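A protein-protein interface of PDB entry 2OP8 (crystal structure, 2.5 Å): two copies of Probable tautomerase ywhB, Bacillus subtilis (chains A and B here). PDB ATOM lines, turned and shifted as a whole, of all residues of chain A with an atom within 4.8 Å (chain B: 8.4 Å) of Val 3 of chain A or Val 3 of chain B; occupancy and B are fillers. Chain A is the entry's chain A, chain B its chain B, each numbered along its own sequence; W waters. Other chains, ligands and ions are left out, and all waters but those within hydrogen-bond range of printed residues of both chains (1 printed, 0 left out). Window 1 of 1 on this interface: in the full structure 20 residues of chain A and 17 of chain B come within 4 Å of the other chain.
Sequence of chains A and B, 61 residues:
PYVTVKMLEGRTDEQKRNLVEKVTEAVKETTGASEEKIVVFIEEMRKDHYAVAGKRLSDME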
ATOM      1  N   PRO A   1       6.400   3.829  12.479  1.00  0.00           N
ATOM      2  CA  PRO A   1       6.545   2.355  12.463  1.00  0.00           C
ATOM      3  C   PRO A   1       7.114   1.852  13.787  1.00  0.00           C
ATOM      4  O   PRO A   1       8.025   2.463  14.351  1.00  0.00           O
ATOM      5  CB  PRO A   1       7.481   2.015  11.312  1.00  0.00           C
ATOM      6  CG  PRO A   1       7.254   3.220  10.380  1.00  0.00           C
ATOM      7  CD  PRO A   1       7.126   4.414  11.336  1.00  0.00           C
ATOM      8  N   TYR A   2       6.570   0.738  14.275  1.00  0.00           N
ATOM      9  CA  TYR A   2       7.014   0.146  15.529  1.00  0.00           C
ATOM     10  C   TYR A   2       7.660  -1.196  15.287  1.00  0.00           C
ATOM     11  O   TYR A   2       7.026  -2.126  14.783  1.00  0.00           O
ATOM     12  CB  TYR A   2       5.839  -0.001  16.490  1.00  0.00           C
ATOM     13  CG  TYR A   2       5.225   1.330  16.819  1.00  0.00           C
ATOM     14  CD1 TYR A   2       4.289   1.920  15.964  1.00  0.00           C
ATOM     15  CD2 TYR A   2       5.641   2.045  17.939  1.00  0.00           C
ATOM     16  CE1 TYR A   2       3.787   3.198  16.217  1.00  0.00           C
ATOM     17  CE2 TYR A   2       5.151   3.319  18.199  1.00  0.00           C
ATOM     18  CZ  TYR A   2       4.227   3.892  17.337  1.00  0.00           C
ATOM     19  OH  TYR A   2       3.761   5.162  17.596  1.00  0.00           O
ATOM     20  N   VAL A   3       8.933  -1.287  15.650  1.00  0.00           N
ATOM     21  CA  VAL A   3       9.690  -2.513  15.466  1.00  0.00           C
ATOM     22  C   VAL A   3      10.057  -3.182  16.785  1.00  0.00           C
ATOM     23  O   VAL A   3      10.685  -2.580  17.660  1.00  0.00           O
ATOM     24  CB  VAL A   3      10.987  -2.242  14.686  1.00  0.00           C
ATOM     25  CG1 VAL A   3      11.779  -3.527  14.521  1.00  0.00           C
ATOM     26  CG2 VAL A   3      10.649  -1.632  13.340  1.00  0.00           C
ATOM     27  N   THR A   4       9.645  -4.434  16.919  1.00  0.00           N
ATOM     28  CA  THR A   4       9.950  -5.199  18.103  1.00  0.00           C
ATOM     29  C   THR A   4      10.937  -6.278  17.679  1.00  0.00           C
ATOM     30  O   THR A   4      10.702  -7.007  16.715  1.00  0.00           O
ATOM     31  CB  THR A   4       8.693  -5.852  18.681  1.00  0.00           C
ATOM     32  OG1 THR A   4       7.772  -4.830  19.074  1.00  0.00           O
ATOM     33  CG2 THR A   4       9.042  -6.698  19.897  1.00  0.00           C
ATOM     34  N   VAL A   5      12.055  -6.350  18.391  1.00  0.00           N
ATOM     35  CA  VAL A   5      13.070  -7.346  18.108  1.00  0.00           C
ATOM     36  C   VAL A   5      13.143  -8.278  19.309  1.00  0.00           C
ATOM     37  O   VAL A   5      13.530  -7.866  20.404  1.00  0.00           O
ATOM     38  CB  VAL A   5      14.452  -6.697  17.874  1.00  0.00           C
ATOM     39  CG1 VAL A   5      15.493  -7.779  17.592  1.00  0.00           C
ATOM     40  CG2 VAL A   5      14.379  -5.730  16.705  1.00  0.00           C
ATOM     41  N   VAL A  23      18.657  -1.353  12.236  1.00  0.00           N
ATOM     42  CA  VAL A  23      17.242  -1.638  12.004  1.00  0.00           C
ATOM     43  C   VAL A  23      16.432  -0.380  11.696  1.00  0.00           C
ATOM     44  O   VAL A  23      15.563  -0.392  10.825  1.00  0.00           O
ATOM     45  CB  VAL A  23      16.618  -2.366  13.223  1.00  0.00           C
ATOM     46  CG1 VAL A  23      15.095  -2.227  13.217  1.00  0.00           C
ATOM     47  CG2 VAL A  23      16.997  -3.835  13.177  1.00  0.00           C
ATOM     48  N   VAL A  27      14.494   0.415   8.024  1.00  0.00           N
ATOM     49  CA  VAL A  27      13.086   0.788   7.931  1.00  0.00           C
ATOM     50  C   VAL A  27      12.896   2.151   7.281  1.00  0.00           C
ATOM     51  O   VAL A  27      11.964   2.356   6.499  1.00  0.00           O
ATOM     52  CB  VAL A  27      12.427   0.816   9.334  1.00  0.00           C
ATOM     53  CG1 VAL A  27      11.004   1.360   9.243  1.00  0.00           C
ATOM     54  CG2 VAL A  27      12.415  -0.575   9.925  1.00  0.00           C
ATOM     55  N   VAL A  39      10.199   3.639  15.964  1.00  0.00           N
ATOM     56  CA  VAL A  39      10.433   3.185  17.334  1.00  0.00           C
ATOM     57  C   VAL A  39      10.891   1.727  17.365  1.00  0.00           C
ATOM     58  O   VAL A  39      10.352   0.883  16.640  1.00  0.00           O
ATOM     59  CB  VAL A  39       9.140   3.308  18.186  1.00  0.00           C
ATOM     60  CG1 VAL A  39       9.352   2.694  19.578  1.00  0.00           C
ATOM     61  CG2 VAL A  39       8.739   4.770  18.306  1.00  0.00           C
ATOM     62  N   VAL A  40      11.884   1.437  18.207  1.00  0.00           N
ATOM     63  CA  VAL A  40      12.401   0.079  18.339  1.00  0.00           C
ATOM     64  C   VAL A  40      12.364  -0.441  19.779  1.00  0.00           C
ATOM     65  O   VAL A  40      12.784   0.249  20.712  1.00  0.00           O
ATOM     66  CB  VAL A  40      13.851  -0.025  17.832  1.00  0.00           C
ATOM     67  CG1 VAL A  40      14.319  -1.456  17.915  1.00  0.00           C
ATOM     68  CG2 VAL A  40      13.943   0.459  16.402  1.00  0.00           C
ATOM     69  N   PHE A  41      11.843  -1.659  19.946  1.00  0.00           N
ATOM     70  CA  PHE A  41      11.764  -2.309  21.251  1.00  0.00           C
ATOM     71  C   PHE A  41      12.604  -3.564  21.184  1.00  0.00           C
ATOM     72  O   PHE A  41      12.545  -4.309  20.200  1.00  0.00           O
ATOM     73  CB  PHE A  41      10.340  -2.758  21.612  1.00  0.00           C
ATOM     74  CG  PHE A  41       9.324  -1.654  21.626  1.00  0.00           C
ATOM     75  CD1 PHE A  41       8.492  -1.442  20.528  1.00  0.00           C
ATOM     76  CD2 PHE A  41       9.187  -0.829  22.739  1.00  0.00           C
ATOM     77  CE1 PHE A  41       7.536  -0.421  20.539  1.00  0.00           C
ATOM     78  CE2 PHE A  41       8.234   0.194  22.757  1.00  0.00           C
ATOM     79  CZ  PHE A  41       7.411   0.398  21.660  1.00  0.00           C
ATOM     80  N   PRO B   1      16.336 -14.871  15.828  1.00  0.00           N
ATOM     81  CA  PRO B   1      15.548 -13.748  16.371  1.00  0.00           C
ATOM     82  C   PRO B   1      14.273 -13.444  15.593  1.00  0.00           C
ATOM     83  O   PRO B   1      14.147 -13.796  14.421  1.00  0.00           O
ATOM     84  CB  PRO B   1      16.474 -12.535  16.423  1.00  0.00           C
ATOM     85  CG  PRO B   1      17.653 -12.981  15.573  1.00  0.00           C
ATOM     86  CD  PRO B   1      17.751 -14.479  15.742  1.00  0.00           C
ATOM     87  N   TYR B   2      13.327 -12.797  16.267  1.00  0.00           N
ATOM     88  CA  TYR B   2      12.049 -12.457  15.663  1.00  0.00           C
ATOM     89  C   TYR B   2      11.805 -10.972  15.634  1.00  0.00           C
ATOM     90  O   TYR B   2      11.803 -10.308  16.668  1.00  0.00           O
ATOM     91  CB  TYR B   2      10.920 -13.133  16.415  1.00  0.00           C
ATOM     92  CG  TYR B   2      11.136 -14.604  16.514  1.00  0.00           C
ATOM     93  CD1 TYR B   2      11.966 -15.143  17.504  1.00  0.00           C
ATOM     94  CD2 TYR B   2      10.566 -15.467  15.586  1.00  0.00           C
ATOM     95  CE1 TYR B   2      12.220 -16.513  17.560  1.00  0.00           C
ATOM     96  CE2 TYR B   2      10.813 -16.827  15.631  1.00  0.00           C
ATOM     97  CZ  TYR B   2      11.639 -17.348  16.615  1.00  0.00           C
ATOM     98  OH  TYR B   2      11.884 -18.704  16.640  1.00  0.00           O
ATOM     99  N   VAL B   3      11.591 -10.464  14.430  1.00  0.00           N
ATOM    100  CA  VAL B   3      11.349  -9.050  14.232  1.00  0.00           C
ATOM    101  C   VAL B   3       9.943  -8.826  13.718  1.00  0.00           C
ATOM    102  O   VAL B   3       9.535  -9.394  12.703  1.00  0.00           O
ATOM    103  CB  VAL B   3      12.331  -8.452  13.210  1.00  0.00           C
ATOM    104  CG1 VAL B   3      12.125  -6.952  13.106  1.00  0.00           C
ATOM    105  CG2 VAL B   3      13.752  -8.777  13.614  1.00  0.00           C
ATOM    106  N   THR B   4       9.198  -8.007  14.446  1.00  0.00           N
ATOM    107  CA  THR B   4       7.852  -7.665  14.050  1.00  0.00           C
ATOM    108  C   THR B   4       7.879  -6.185  13.693  1.00  0.00           C
ATOM    109  O   THR B   4       8.335  -5.349  14.483  1.00  0.00           O
ATOM    110  CB  THR B   4       6.834  -7.872  15.187  1.00  0.00           C
ATOM    111  OG1 THR B   4       6.800  -9.253  15.560  1.00  0.00           O
ATOM    112  CG2 THR B   4       5.441  -7.441  14.733  1.00  0.00           C
ATOM    113  N   VAL B   5       7.420  -5.870  12.488  1.00  0.00           N
ATOM    114  CA  VAL B   5       7.357  -4.488  12.047  1.00  0.00           C
ATOM    115  C   VAL B   5       5.881  -4.119  11.934  1.00  0.00           C
ATOM    116  O   VAL B   5       5.135  -4.726  11.166  1.00  0.00           O
ATOM    117  CB  VAL B   5       8.029  -4.292  10.678  1.00  0.00           C
ATOM    118  CG1 VAL B   5       7.957  -2.815  10.278  1.00  0.00           C
ATOM    119  CG2 VAL B   5       9.482  -4.762  10.734  1.00  0.00           C
ATOM    120  N   LYS B   6       5.466  -3.130  12.716  1.00  0.00           N
ATOM    121  CA  LYS B   6       4.083  -2.669  12.724  1.00  0.00           C
ATOM    122  C   LYS B   6       4.053  -1.264  12.090  1.00  0.00           C
ATOM    123  O   LYS B   6       4.708  -0.340  12.579  1.00  0.00           O
ATOM    124  CB  LYS B   6       3.577  -2.636  14.175  1.00  0.00           C
ATOM    125  CG  LYS B   6       2.073  -2.592  14.347  1.00  0.00           C
ATOM    126  CD  LYS B   6       1.666  -2.635  15.823  1.00  0.00           C
ATOM    127  CE  LYS B   6       0.145  -2.683  15.941  1.00  0.00           C
ATOM    128  NZ  LYS B   6      -0.367  -2.692  17.346  1.00  0.00           N
ATOM    129  N   MET B   7       3.315  -1.115  10.990  1.00  0.00           N
ATOM    130  CA  MET B   7       3.209   0.172  10.301  1.00  0.00           C
ATOM    131  C   MET B   7       1.850   0.331   9.627  1.00  0.00           C
ATOM    132  O   MET B   7       1.114  -0.645   9.448  1.00  0.00           O
ATOM    133  CB  MET B   7       4.310   0.296   9.247  1.00  0.00           C
ATOM    134  CG  MET B   7       4.243  -0.791   8.180  1.00  0.00           C
ATOM    135  SD  MET B   7       5.543  -0.678   6.924  1.00  0.00           S
ATOM    136  CE  MET B   7       5.088  -2.089   5.885  1.00  0.00           C
ATOM    137  N   LEU B  19      11.847  -4.194   2.855  1.00  0.00           N
ATOM    138  CA  LEU B  19      11.825  -4.074   4.300  1.00  0.00           C
ATOM    139  C   LEU B  19      12.359  -5.371   4.894  1.00  0.00           C
ATOM    140  O   LEU B  19      13.313  -5.366   5.663  1.00  0.00           O
ATOM    141  CB  LEU B  19      10.396  -3.841   4.775  1.00  0.00           C
ATOM    142  CG  LEU B  19      10.183  -3.778   6.290  1.00  0.00           C
ATOM    143  CD1 LEU B  19      10.930  -2.591   6.901  1.00  0.00           C
ATOM    144  CD2 LEU B  19       8.700  -3.669   6.556  1.00  0.00           C
ATOM    145  N   VAL B  20      11.738  -6.481   4.516  1.00  0.00           N
ATOM    146  CA  VAL B  20      12.132  -7.791   5.005  1.00  0.00           C
ATOM    147  C   VAL B  20      13.612  -8.048   4.772  1.00  0.00           C
ATOM    148  O   VAL B  20      14.325  -8.510   5.666  1.00  0.00           O
ATOM    149  CB  VAL B  20      11.317  -8.897   4.310  1.00  0.00           C
ATOM    150  CG1 VAL B  20      11.986 -10.239   4.500  1.00  0.00           C
ATOM    151  CG2 VAL B  20       9.924  -8.934   4.882  1.00  0.00           C
ATOM    152  N   VAL B  23      15.881  -5.263   6.774  1.00  0.00           N
ATOM    153  CA  VAL B  23      15.775  -5.523   8.198  1.00  0.00           C
ATOM    154  C   VAL B  23      16.491  -6.805   8.594  1.00  0.00           C
ATOM    155  O   VAL B  23      17.121  -6.861   9.645  1.00  0.00           O
ATOM    156  CB  VAL B  23      14.303  -5.586   8.632  1.00  0.00           C
ATOM    157  CG1 VAL B  23      14.171  -6.302   9.956  1.00  0.00           C
ATOM    158  CG2 VAL B  23      13.768  -4.183   8.764  1.00  0.00           C
ATOM    159  N   THR B  24      16.397  -7.831   7.753  1.00  0.00           N
ATOM    160  CA  THR B  24      17.060  -9.098   8.043  1.00  0.00           C
ATOM    161  C   THR B  24      18.586  -8.955   8.033  1.00  0.00           C
ATOM    162  O   THR B  24      19.273  -9.519   8.887  1.00  0.00           O
ATOM    163  CB  THR B  24      16.653 -10.186   7.035  1.00  0.00           C
ATOM    164  OG1 THR B  24      15.248 -10.453   7.153  1.00  0.00           O
ATOM    165  CG2 THR B  24      17.435 -11.467   7.294  1.00  0.00           C
ATOM    166  N   ALA B  26      20.203  -6.211   8.597  1.00  0.00           N
ATOM    167  CA  ALA B  26      20.530  -5.361   9.735  1.00  0.00           C
ATOM    168  C   ALA B  26      20.648  -6.185  11.018  1.00  0.00           C
ATOM    169  O   ALA B  26      21.455  -5.877  11.894  1.00  0.00           O
ATOM    170  CB  ALA B  26      19.463  -4.283   9.905  1.00  0.00           C
ATOM    171  N   VAL B  27      19.835  -7.233  11.122  1.00  0.00           N
ATOM    172  CA  VAL B  27      19.846  -8.103  12.290  1.00  0.00           C
ATOM    173  C   VAL B  27      21.057  -9.019  12.215  1.00  0.00           C
ATOM    174  O   VAL B  27      21.826  -9.137  13.171  1.00  0.00           O
ATOM    175  CB  VAL B  27      18.545  -8.960  12.364  1.00  0.00           C
ATOM    176  CG1 VAL B  27      18.675 -10.037  13.442  1.00  0.00           C
ATOM    177  CG2 VAL B  27      17.345  -8.062  12.661  1.00  0.00           C
ATOM    178  N   LYS B  28      21.213  -9.663  11.065  1.00  0.00           N
ATOM    179  CA  LYS B  28      22.322 -10.578  10.806  1.00  0.00           C
ATOM    180  C   LYS B  28      23.686  -9.964  11.132  1.00  0.00           C
ATOM    181  O   LYS B  28      24.480 -10.536  11.875  1.00  0.00           O
ATOM    182  CB  LYS B  28      22.295 -10.986   9.332  1.00  0.00           C
ATOM    183  CG  LYS B  28      23.458 -11.850   8.875  1.00  0.00           C
ATOM    184  CD  LYS B  28      23.541 -11.858   7.350  1.00  0.00           C
ATOM    185  CE  LYS B  28      24.579 -12.849   6.828  1.00  0.00           C
ATOM    186  NZ  LYS B  28      24.174 -14.263   7.070  1.00  0.00           N
ATOM    187  N   THR B  31      23.892  -8.732  15.249  1.00  0.00           N
ATOM    188  CA  THR B  31      23.718  -9.631  16.392  1.00  0.00           C
ATOM    189  C   THR B  31      24.456 -10.955  16.247  1.00  0.00           C
ATOM    190  O   THR B  31      24.600 -11.703  17.219  1.00  0.00           O
ATOM    191  CB  THR B  31      22.238  -9.985  16.614  1.00  0.00           C
ATOM    192  OG1 THR B  31      21.798 -10.881  15.578  1.00  0.00           O
ATOM    193  CG2 THR B  31      21.390  -8.733  16.601  1.00  0.00           C
ATOM    194  N   LYS B  37      17.660 -18.201  10.784  1.00  0.00           N
ATOM    195  CA  LYS B  37      17.206 -18.113  12.164  1.00  0.00           C
ATOM    196  C   LYS B  37      16.588 -16.732  12.397  1.00  0.00           C
ATOM    197  O   LYS B  37      16.196 -16.396  13.514  1.00  0.00           O
ATOM    198  CB  LYS B  37      18.380 -18.328  13.123  1.00  0.00           C
ATOM    199  CG  LYS B  37      19.027 -19.706  13.051  1.00  0.00           C
ATOM    200  N   ILE B  38      16.507 -15.931  11.338  1.00  0.00           N
ATOM    201  CA  ILE B  38      15.929 -14.597  11.433  1.00  0.00           C
ATOM    202  C   ILE B  38      14.547 -14.573  10.777  1.00  0.00           C
ATOM    203  O   ILE B  38      14.411 -14.833   9.579  1.00  0.00           O
ATOM    204  CB  ILE B  38      16.828 -13.557  10.747  1.00  0.00           C
ATOM    205  CG1 ILE B  38      18.209 -13.544  11.413  1.00  0.00           C
ATOM    206  CG2 ILE B  38      16.171 -12.174  10.819  1.00  0.00           C
ATOM    207  CD1 ILE B  38      19.193 -12.567  10.779  1.00  0.00           C
ATOM    208  N   VAL B  39      13.525 -14.262  11.574  1.00  0.00           N
ATOM    209  CA  VAL B  39      12.146 -14.214  11.099  1.00  0.00           C
ATOM    210  C   VAL B  39      11.577 -12.800  11.181  1.00  0.00           C
ATOM    211  O   VAL B  39      11.785 -12.093  12.168  1.00  0.00           O
ATOM    212  CB  VAL B  39      11.250 -15.149  11.930  1.00  0.00           C
ATOM    213  CG1 VAL B  39       9.805 -15.068  11.460  1.00  0.00           C
ATOM    214  CG2 VAL B  39      11.757 -16.564  11.815  1.00  0.00           C
ATOM    215  N   VAL B  40      10.858 -12.392  10.139  1.00  0.00           N
ATOM    216  CA  VAL B  40      10.262 -11.069  10.119  1.00  0.00           C
ATOM    217  C   VAL B  40       8.755 -11.128   9.910  1.00  0.00           C
ATOM    218  O   VAL B  40       8.269 -11.774   8.984  1.00  0.00           O
ATOM    219  CB  VAL B  40      10.867 -10.198   9.006  1.00  0.00           C
ATOM    220  CG1 VAL B  40      10.225  -8.828   9.026  1.00  0.00           C
ATOM    221  CG2 VAL B  40      12.370 -10.072   9.201  1.00  0.00           C
ATOM    222  N   PHE B  41       8.016 -10.463  10.789  1.00  0.00           N
ATOM    223  CA  PHE B  41       6.565 -10.412  10.683  1.00  0.00           C
ATOM    224  C   PHE B  41       6.201  -8.986  10.313  1.00  0.00           C
ATOM    225  O   PHE B  41       6.774  -8.035  10.843  1.00  0.00           O
ATOM    226  CB  PHE B  41       5.880 -10.727  12.017  1.00  0.00           C
ATOM    227  CG  PHE B  41       6.220 -12.068  12.583  1.00  0.00           C
ATOM    228  CD1 PHE B  41       7.319 -12.226  13.426  1.00  0.00           C
ATOM    229  CD2 PHE B  41       5.432 -13.178  12.289  1.00  0.00           C
ATOM    230  CE1 PHE B  41       7.626 -13.480  13.972  1.00  0.00           C
ATOM    231  CE2 PHE B  41       5.729 -14.431  12.828  1.00  0.00           C
ATOM    232  CZ  PHE B  41       6.827 -14.582  13.671  1.00  0.00           C
ATOM    233  N   ILE B  42       5.257  -8.841   9.394  1.00  0.00           N
ATOM    234  CA  ILE B  42       4.799  -7.519   9.006  1.00  0.00           C
ATOM    235  C   ILE B  42       3.355  -7.374   9.479  1.00  0.00           C
ATOM    236  O   ILE B  42       2.519  -8.238   9.209  1.00  0.00           O
ATOM    237  CB  ILE B  42       4.842  -7.316   7.483  1.00  0.00           C
ATOM    238  CG1 ILE B  42       6.282  -7.446   6.980  1.00  0.00           C
ATOM    239  CG2 ILE B  42       4.294  -5.939   7.134  1.00  0.00           C
ATOM    240  CD1 ILE B  42       6.432  -7.352   5.455  1.00  0.00           C
ATOM    241  N   GLU B  43       3.077  -6.295  10.204  1.00  0.00           N
ATOM    242  CA  GLU B  43       1.735  -6.022  10.708  1.00  0.00           C
ATOM    243  C   GLU B  43       1.300  -4.624  10.283  1.00  0.00           C
ATOM    244  O   GLU B  43       1.961  -3.628  10.596  1.00  0.00           O
ATOM    245  CB  GLU B  43       1.704  -6.155  12.231  1.00  0.00           C
ATOM    246  CG  GLU B  43       1.673  -7.602  12.699  1.00  0.00           C
ATOM    247  CD  GLU B  43       1.901  -7.746  14.186  1.00  0.00           C
ATOM    248  OE1 GLU B  43       1.452  -6.863  14.948  1.00  0.00           O
ATOM    249  OE2 GLU B  43       2.524  -8.752  14.589  1.00  0.00           O
HETATM  250  O   HOH W   1       6.456  -4.104  16.873  1.00  0.00           O
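Of the printed residues of chain B, Val 3 of chain A touches Val 3 (3.7 Å) and Thr 4 (3.3 Å).
Val 3 of chain B touches two residues of chain A.
Of the printed residues of chain B, Val 5 of chain A touches Tyr 2 (3.5 Å).
Of the printed residues of chain B, Tyr 2 of chain A touches Thr 4 (3.5 Å), Val 5 (3.6 Å) and Lys 6 (2.7 Å).
Val 23 of chain B touches none of the printed residues of chain A.
The nearest residue of chain B that does not touch Val 3 of chain A is Val 5 of chain B (4.2 Å).
Tyr 2 of chain A touches Thr 4 of chain B, and with the chains exchanged Thr 4 of chain A touches Tyr 2 of chain B.
Tyr 2 of chain A touches Val 5 of chain B, and with the chains exchanged Val 5 of chain A touches Tyr 2 of chain B.
Val 3 of chain A touches its own counterpart, Val 3 of chain B.
Val 3 of chain A touches Thr 4 of chain B, and with the chains exchanged Thr 4 of chain A touches Val 3 of chain B.
Positions printed for both chains: 1, 2, 3, 4, 5, 23, 27, 39, 40 and 41.
Water W1 lies within hydrogen-bond range of the side-chain hydroxyl (OG1) of Thr 4 of chain A (2.7 Å), the backbone carbonyl oxygen (O) of Tyr 2 of chain A (2.9 Å) and the backbone carbonyl oxygen (O) of Thr 4 of chain B (3.3 Å).
The backbone carbonyl oxygen (O) of Lys 6 of chain B is in hydrogen-bond range of the backbone NH (N) of Tyr 2 of chain A.
O of Thr 4 of chain A is in hydrogen-bond range of N of Thr 4 of chain B, 2.9 Å away.
O of Thr 4 of chain B sits close to O of Tyr 2 of chain A.
O of Thr 4 of chain A sits close to O of Tyr 2 of chain B, 3.5 Å away.
Of the 10 printed residues of chain A, 7 touch a printed residue of chain B.
Among the printed residues, 12 pairs touch across the chains.
O of Lys 6 of chain B touches CA of Pro 1 of chain A (3.3 Å).
Tyr 2 of chain A touches Val 5 of chain B (O to CA, 3.6 Å).
CG1 of Val 3 of chain A touches CG1 of Val 3 of chain B (3.7 Å).
Thr 4 of chain B touches Val 3 of chain A (O to CA, 3.3 Å).
Thr 4 of chain A touches Val 3 of chain B.
Val 5 of chain A touches Tyr 2 of chain B.
N of Val 23 of chain A touches CB of Ala 26 of chain B (3.8 Å).
Leu 19 of chain B touches Val 27 of chain A.
O of Pro 1 of chain A lies within hydrogen-bond range of N of Val 39 of chain A.
N of Val 3 of chain A sits at hydrogen-bond distance from O of Val 39 of chain A (2.8 Å).
The backbone NH of Phe 41 of chain A sits at hydrogen-bond distance from the backbone carbonyl oxygen of Val 3 of chain A (2.7 Å).
The backbone carbonyl oxygen of Val 3 of chain B lies within hydrogen-bond range of the backbone NH of Phe 41 of chain B (2.7 Å).
The backbone NH (N) of Val 5 of chain B sits at hydrogen-bond distance from the backbone carbonyl oxygen (O) of Phe 41 of chain B, at 2.8 Å.
N of Glu 43 of chain B is in hydrogen-bond range of O of Val 5 of chain B.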
